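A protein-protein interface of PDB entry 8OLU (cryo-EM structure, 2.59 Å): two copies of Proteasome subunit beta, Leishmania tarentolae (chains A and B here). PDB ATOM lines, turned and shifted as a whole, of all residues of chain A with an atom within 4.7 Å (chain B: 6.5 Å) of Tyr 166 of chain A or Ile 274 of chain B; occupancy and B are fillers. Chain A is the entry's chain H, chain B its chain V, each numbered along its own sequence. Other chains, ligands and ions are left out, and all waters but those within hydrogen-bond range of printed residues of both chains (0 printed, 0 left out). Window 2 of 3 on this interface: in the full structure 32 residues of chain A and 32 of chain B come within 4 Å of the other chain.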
ATOM      1  N   VAL A 130       4.064 -14.936 -26.476  1.00  0.00           N
ATOM      2  CA  VAL A 130       2.976 -14.062 -26.762  1.00  0.00           C
ATOM      3  C   VAL A 130       3.002 -12.921 -25.767  1.00  0.00           C
ATOM      4  O   VAL A 130       2.757 -11.768 -26.085  1.00  0.00           O
ATOM      5  CB  VAL A 130       1.666 -14.823 -26.773  1.00  0.00           C
ATOM      6  CG1 VAL A 130       0.517 -13.890 -27.062  1.00  0.00           C
ATOM      7  CG2 VAL A 130       1.672 -15.948 -27.772  1.00  0.00           C
ATOM      8  N   ALA A 131       3.388 -13.211 -24.566  1.00  0.00           N
ATOM      9  CA  ALA A 131       3.556 -12.157 -23.595  1.00  0.00           C
ATOM     10  C   ALA A 131       4.480 -11.042 -24.085  1.00  0.00           C
ATOM     11  O   ALA A 131       4.220  -9.879 -23.874  1.00  0.00           O
ATOM     12  CB  ALA A 131       4.083 -12.731 -22.317  1.00  0.00           C
ATOM     13  N   ALA A 134       2.475  -8.980 -26.475  1.00  0.00           N
ATOM     14  CA  ALA A 134       1.454  -8.223 -25.805  1.00  0.00           C
ATOM     15  C   ALA A 134       2.060  -7.089 -25.022  1.00  0.00           C
ATOM     16  O   ALA A 134       1.526  -6.009 -24.896  1.00  0.00           O
ATOM     17  CB  ALA A 134       0.770  -9.088 -24.824  1.00  0.00           C
ATOM     18  N   ILE A 152      -6.823  -3.677 -29.291  1.00  0.00           N
ATOM     19  CA  ILE A 152      -6.040  -4.769 -29.821  1.00  0.00           C
ATOM     20  C   ILE A 152      -6.341  -6.055 -29.075  1.00  0.00           C
ATOM     21  O   ILE A 152      -6.812  -6.077 -27.986  1.00  0.00           O
ATOM     22  CB  ILE A 152      -4.570  -4.358 -29.678  1.00  0.00           C
ATOM     23  CG1 ILE A 152      -4.323  -3.081 -30.468  1.00  0.00           C
ATOM     24  CG2 ILE A 152      -3.586  -5.394 -30.130  1.00  0.00           C
ATOM     25  CD1 ILE A 152      -4.597  -3.314 -31.943  1.00  0.00           C
ATOM     26  N   ILE A 153      -6.177  -7.133 -29.748  1.00  0.00           N
ATOM     27  CA  ILE A 153      -6.084  -8.376 -29.089  1.00  0.00           C
ATOM     28  C   ILE A 153      -4.830  -8.967 -29.629  1.00  0.00           C
ATOM     29  O   ILE A 153      -4.565  -8.840 -30.782  1.00  0.00           O
ATOM     30  CB  ILE A 153      -7.245  -9.289 -29.440  1.00  0.00           C
ATOM     31  CG1 ILE A 153      -8.509  -8.712 -28.836  1.00  0.00           C
ATOM     32  CG2 ILE A 153      -6.989 -10.704 -28.946  1.00  0.00           C
ATOM     33  CD1 ILE A 153      -9.782  -9.348 -29.283  1.00  0.00           C
ATOM     34  N   VAL A 154      -4.044  -9.554 -28.769  1.00  0.00           N
ATOM     35  CA  VAL A 154      -2.830 -10.168 -29.194  1.00  0.00           C
ATOM     36  C   VAL A 154      -2.992 -11.578 -28.780  1.00  0.00           C
ATOM     37  O   VAL A 154      -3.329 -11.828 -27.673  1.00  0.00           O
ATOM     38  CB  VAL A 154      -1.599  -9.559 -28.554  1.00  0.00           C
ATOM     39  CG1 VAL A 154      -0.384 -10.329 -28.957  1.00  0.00           C
ATOM     40  CG2 VAL A 154      -1.458  -8.117 -28.989  1.00  0.00           C
ATOM     41  N   ASN A 161       4.172 -21.272 -23.120  1.00  0.00           N
ATOM     42  CA  ASN A 161       2.902 -20.986 -22.487  1.00  0.00           C
ATOM     43  C   ASN A 161       1.693 -21.483 -23.263  1.00  0.00           C
ATOM     44  O   ASN A 161       0.563 -21.227 -22.859  1.00  0.00           O
ATOM     45  CB  ASN A 161       2.757 -19.501 -22.266  1.00  0.00           C
ATOM     46  CG  ASN A 161       3.540 -19.103 -21.064  1.00  0.00           C
ATOM     47  OD1 ASN A 161       3.528 -19.845 -20.084  1.00  0.00           O
ATOM     48  ND2 ASN A 161       4.292 -18.040 -21.169  1.00  0.00           N
ATOM     49  N   SER A 164      -2.197 -18.145 -25.964  1.00  0.00           N
ATOM     50  CA  SER A 164      -2.570 -17.090 -25.076  1.00  0.00           C
ATOM     51  C   SER A 164      -3.324 -16.021 -25.801  1.00  0.00           C
ATOM     52  O   SER A 164      -3.070 -15.762 -26.950  1.00  0.00           O
ATOM     53  CB  SER A 164      -1.352 -16.456 -24.521  1.00  0.00           C
ATOM     54  OG  SER A 164      -0.654 -17.282 -23.554  1.00  0.00           O
ATOM     55  N   VAL A 165      -4.027 -15.214 -25.022  1.00  0.00           N
ATOM     56  CA  VAL A 165      -4.858 -14.150 -25.532  1.00  0.00           C
ATOM     57  C   VAL A 165      -4.698 -12.982 -24.627  1.00  0.00           C
ATOM     58  O   VAL A 165      -4.926 -13.087 -23.445  1.00  0.00           O
ATOM     59  CB  VAL A 165      -6.313 -14.607 -25.529  1.00  0.00           C
ATOM     60  CG1 VAL A 165      -7.272 -13.554 -25.998  1.00  0.00           C
ATOM     61  CG2 VAL A 165      -6.456 -15.773 -26.432  1.00  0.00           C
ATOM     62  N   TYR A 166      -4.451 -11.847 -25.198  1.00  0.00           N
ATOM     63  CA  TYR A 166      -4.371 -10.676 -24.380  1.00  0.00           C
ATOM     64  C   TYR A 166      -5.277  -9.655 -24.981  1.00  0.00           C
ATOM     65  O   TYR A 166      -5.270  -9.531 -26.150  1.00  0.00           O
ATOM     66  CB  TYR A 166      -2.959 -10.110 -24.342  1.00  0.00           C
ATOM     67  CG  TYR A 166      -1.977 -10.980 -23.645  1.00  0.00           C
ATOM     68  CD1 TYR A 166      -1.497 -12.096 -24.258  1.00  0.00           C
ATOM     69  CD2 TYR A 166      -1.571 -10.737 -22.341  1.00  0.00           C
ATOM     70  CE1 TYR A 166      -0.645 -12.964 -23.606  1.00  0.00           C
ATOM     71  CE2 TYR A 166      -0.629 -11.549 -21.705  1.00  0.00           C
ATOM     72  CZ  TYR A 166      -0.162 -12.668 -22.355  1.00  0.00           C
ATOM     73  OH  TYR A 166       0.717 -13.568 -21.812  1.00  0.00           O
ATOM     74  N   SER A 167      -5.991  -8.929 -24.183  1.00  0.00           N
ATOM     75  CA  SER A 167      -6.782  -7.840 -24.650  1.00  0.00           C
ATOM     76  C   SER A 167      -6.073  -6.579 -24.347  1.00  0.00           C
ATOM     77  O   SER A 167      -5.693  -6.378 -23.224  1.00  0.00           O
ATOM     78  CB  SER A 167      -8.039  -7.818 -23.905  1.00  0.00           C
ATOM     79  OG  SER A 167      -8.958  -6.878 -24.490  1.00  0.00           O
ATOM     80  N   ILE A 168      -5.907  -5.713 -25.283  1.00  0.00           N
ATOM     81  CA  ILE A 168      -5.362  -4.438 -24.916  1.00  0.00           C
ATOM     82  C   ILE A 168      -6.330  -3.375 -25.331  1.00  0.00           C
ATOM     83  O   ILE A 168      -6.322  -2.912 -26.446  1.00  0.00           O
ATOM     84  CB  ILE A 168      -4.026  -4.241 -25.601  1.00  0.00           C
ATOM     85  CG1 ILE A 168      -3.007  -5.236 -25.071  1.00  0.00           C
ATOM     86  CG2 ILE A 168      -3.516  -2.821 -25.438  1.00  0.00           C
ATOM     87  CD1 ILE A 168      -1.991  -5.537 -26.090  1.00  0.00           C
ATOM     88  N   CYS A 174      -3.502  -4.186 -20.284  1.00  0.00           N
ATOM     89  CA  CYS A 174      -3.263  -5.440 -20.929  1.00  0.00           C
ATOM     90  C   CYS A 174      -3.710  -6.537 -20.006  1.00  0.00           C
ATOM     91  O   CYS A 174      -3.154  -6.681 -18.937  1.00  0.00           O
ATOM     92  CB  CYS A 174      -1.800  -5.602 -21.224  1.00  0.00           C
ATOM     93  SG  CYS A 174      -1.333  -7.214 -21.904  1.00  0.00           S
ATOM     94  N   VAL A 175      -4.654  -7.327 -20.491  1.00  0.00           N
ATOM     95  CA  VAL A 175      -5.245  -8.312 -19.647  1.00  0.00           C
ATOM     96  C   VAL A 175      -5.203  -9.658 -20.309  1.00  0.00           C
ATOM     97  O   VAL A 175      -5.743  -9.810 -21.377  1.00  0.00           O
ATOM     98  CB  VAL A 175      -6.690  -7.946 -19.339  1.00  0.00           C
ATOM     99  CG1 VAL A 175      -7.315  -8.984 -18.478  1.00  0.00           C
ATOM    100  CG2 VAL A 175      -6.738  -6.651 -18.636  1.00  0.00           C
ATOM    101  N   LYS A 176      -4.698 -10.639 -19.574  1.00  0.00           N
ATOM    102  CA  LYS A 176      -4.606 -11.964 -20.113  1.00  0.00           C
ATOM    103  C   LYS A 176      -5.860 -12.791 -19.845  1.00  0.00           C
ATOM    104  O   LYS A 176      -6.128 -13.222 -18.736  1.00  0.00           O
ATOM    105  CB  LYS A 176      -3.470 -12.715 -19.490  1.00  0.00           C
ATOM    106  CG  LYS A 176      -2.999 -13.886 -20.320  1.00  0.00           C
ATOM    107  CD  LYS A 176      -1.976 -14.641 -19.596  1.00  0.00           C
ATOM    108  CE  LYS A 176      -1.479 -15.862 -20.295  1.00  0.00           C
ATOM    109  NZ  LYS A 176      -2.536 -16.868 -20.472  1.00  0.00           N
ATOM    110  N   THR B 263      -4.494 -13.979 -15.090  1.00  0.00           N
ATOM    111  CA  THR B 263      -3.158 -14.074 -14.528  1.00  0.00           C
ATOM    112  C   THR B 263      -2.400 -12.784 -14.813  1.00  0.00           C
ATOM    113  O   THR B 263      -1.798 -12.630 -15.875  1.00  0.00           O
ATOM    114  CB  THR B 263      -2.417 -15.237 -15.164  1.00  0.00           C
ATOM    115  OG1 THR B 263      -3.039 -16.481 -14.870  1.00  0.00           O
ATOM    116  CG2 THR B 263      -1.032 -15.239 -14.601  1.00  0.00           C
ATOM    117  N   GLN B 264      -2.552 -11.823 -13.914  1.00  0.00           N
ATOM    118  CA  GLN B 264      -2.091 -10.470 -14.140  1.00  0.00           C
ATOM    119  C   GLN B 264      -0.960 -10.127 -13.221  1.00  0.00           C
ATOM    120  O   GLN B 264      -0.324  -9.116 -13.404  1.00  0.00           O
ATOM    121  CB  GLN B 264      -3.128  -9.429 -13.742  1.00  0.00           C
ATOM    122  CG  GLN B 264      -4.336  -9.453 -14.613  1.00  0.00           C
ATOM    123  CD  GLN B 264      -4.040  -9.001 -16.020  1.00  0.00           C
ATOM    124  OE1 GLN B 264      -3.887  -9.844 -16.891  1.00  0.00           O
ATOM    125  NE2 GLN B 264      -3.984  -7.697 -16.243  1.00  0.00           N
ATOM    126  N   GLN B 266       1.724 -11.795 -11.908  1.00  0.00           N
ATOM    127  CA  GLN B 266       2.634 -12.907 -11.890  1.00  0.00           C
ATOM    128  C   GLN B 266       3.685 -12.638 -10.850  1.00  0.00           C
ATOM    129  O   GLN B 266       4.082 -11.510 -10.664  1.00  0.00           O
ATOM    130  CB  GLN B 266       3.328 -13.012 -13.230  1.00  0.00           C
ATOM    131  CG  GLN B 266       2.523 -13.691 -14.325  1.00  0.00           C
ATOM    132  CD  GLN B 266       3.326 -13.510 -15.595  1.00  0.00           C
ATOM    133  OE1 GLN B 266       4.511 -13.859 -15.657  1.00  0.00           O
ATOM    134  NE2 GLN B 266       2.723 -12.871 -16.578  1.00  0.00           N
ATOM    135  N   SER B 271      11.744 -17.359 -15.147  1.00  0.00           N
ATOM    136  CA  SER B 271      11.261 -17.912 -16.391  1.00  0.00           C
ATOM    137  C   SER B 271      10.131 -17.061 -16.962  1.00  0.00           C
ATOM    138  O   SER B 271       9.564 -16.197 -16.301  1.00  0.00           O
ATOM    139  CB  SER B 271      10.859 -19.353 -16.227  1.00  0.00           C
ATOM    140  OG  SER B 271      10.247 -19.871 -17.402  1.00  0.00           O
ATOM    141  N   ALA B 272       9.886 -17.275 -18.253  1.00  0.00           N
ATOM    142  CA  ALA B 272       8.737 -16.731 -18.929  1.00  0.00           C
ATOM    143  C   ALA B 272       7.481 -17.589 -18.724  1.00  0.00           C
ATOM    144  O   ALA B 272       6.380 -17.143 -19.080  1.00  0.00           O
ATOM    145  CB  ALA B 272       9.063 -16.616 -20.383  1.00  0.00           C
ATOM    146  N   LYS B 273       7.663 -18.827 -18.245  1.00  0.00           N
ATOM    147  CA  LYS B 273       6.541 -19.711 -17.979  1.00  0.00           C
ATOM    148  C   LYS B 273       5.653 -19.049 -16.931  1.00  0.00           C
ATOM    149  O   LYS B 273       6.105 -18.713 -15.837  1.00  0.00           O
ATOM    150  CB  LYS B 273       7.063 -21.080 -17.549  1.00  0.00           C
ATOM    151  CG  LYS B 273       6.038 -22.074 -17.036  1.00  0.00           C
ATOM    152  CD  LYS B 273       4.825 -22.202 -17.925  1.00  0.00           C
ATOM    153  CE  LYS B 273       3.828 -23.234 -17.434  1.00  0.00           C
ATOM    154  NZ  LYS B 273       4.347 -24.591 -17.724  1.00  0.00           N
ATOM    155  N   ILE B 274       4.412 -18.824 -17.330  1.00  0.00           N
ATOM    156  CA  ILE B 274       3.354 -18.264 -16.527  1.00  0.00           C
ATOM    157  C   ILE B 274       2.714 -19.339 -15.643  1.00  0.00           C
ATOM    158  O   ILE B 274       2.345 -20.420 -16.096  1.00  0.00           O
ATOM    159  CB  ILE B 274       2.349 -17.613 -17.487  1.00  0.00           C
ATOM    160  CG1 ILE B 274       2.881 -16.269 -17.974  1.00  0.00           C
ATOM    161  CG2 ILE B 274       0.999 -17.459 -16.860  1.00  0.00           C
ATOM    162  CD1 ILE B 274       2.151 -15.700 -19.160  1.00  0.00           C
ATOM    163  N   THR B 275       2.564 -18.994 -14.361  1.00  0.00           N
ATOM    164  CA  THR B 275       2.185 -19.951 -13.330  1.00  0.00           C
ATOM    165  C   THR B 275       0.783 -19.609 -12.825  1.00  0.00           C
ATOM    166  O   THR B 275      -0.065 -20.488 -12.679  1.00  0.00           O
ATOM    167  CB  THR B 275       3.257 -20.037 -12.211  1.00  0.00           C
ATOM    168  OG1 THR B 275       3.576 -18.772 -11.613  1.00  0.00           O
ATOM    169  CG2 THR B 275       4.560 -20.624 -12.735  1.00  0.00           C
ATOM    170  N   GLY B 276       0.518 -18.328 -12.587  1.00  0.00           N
ATOM    171  CA  GLY B 276      -0.479 -17.994 -11.596  1.00  0.00           C
ATOM    172  C   GLY B 276      -0.261 -16.606 -11.025  1.00  0.00           C
ATOM    173  O   GLY B 276       0.673 -15.913 -11.369  1.00  0.00           O
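Among the printed residues, pairs that only touch across the chains: Asn 161 of chain A with Lys 273 of chain B, Tyr 166 of chain A with Ile 274 of chain B, Val 175 of chain A with Gln 264 of chain B, Lys 176 of chain A with Thr 263 of chain B and Lys 176 of chain A with Ile 274 of chain B.
The side-chain amide nitrogen (ND2) of Asn 161 of chain A sits at hydrogen-bond distance from the backbone carbonyl oxygen (O) of Ala 272 of chain B (3.1 Å).
OE1 of Gln 264 of chain B lies within hydrogen-bond range of N of Lys 176 of chain A, 2.9 Å away.
The side-chain amide oxygen (OD1) of Asn 161 of chain A is in hydrogen-bond range of the backbone NH (N) of Ile 274 of chain B (3.1 Å).
O of Cys 174 of chain A sits at hydrogen-bond distance from NE2 of Gln 264 of chain B, 3.0 Å away.
Hydrophobic or aromatic side chains of chain B that line the printed part of chain A: Ile 274.
Hydrophobic or aromatic side chains of chain A within 4 Å of the printed part of chain B: Tyr 166 and Val 175.
Along chain A the printed residues that touch a printed residue of chain B span positions 161 to 176.
The backbone NH (N) of Tyr 166 of chain A is in hydrogen-bond range of the backbone carbonyl oxygen (O) of Val 154 of chain A (2.7 Å).
OG of Ser 271 of chain B sits at hydrogen-bond distance from N of Lys 273 of chain B (2.9 Å).
The backbone NH of Ser 167 of chain A lies within hydrogen-bond range of the backbone carbonyl oxygen of Val 175 of chain A (3.0 Å).
Tyr 166 of chain A touches one residue of chain B.
Of the printed residues of chain B, Cys 174 of chain A touches Gln 264.
Of the printed residues of chain B, Val 175 of chain A touches Gln 264 (3.4 Å).
Printed residues of chain A within 4 Å of Thr 263 of chain B: Lys 176 (3.98 Å).
Of the printed residues of chain A, Gln 264 of chain B touches Cys 174, Val 175 and Lys 176.
Printed residues of chain A within 4 Å of Lys 273 of chain B: Asn 161.
Thr 275 of chain B touches none of the printed residues of chain A.
The nearest residue of chain B that does not touch Tyr 166 of chain A is Gln 266 of chain B (5.6 Å).
No position is printed for both chains.
Of the 9 pairs that touch across the chains among the printed residues, none has its exchanged pair printed and touching as well.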
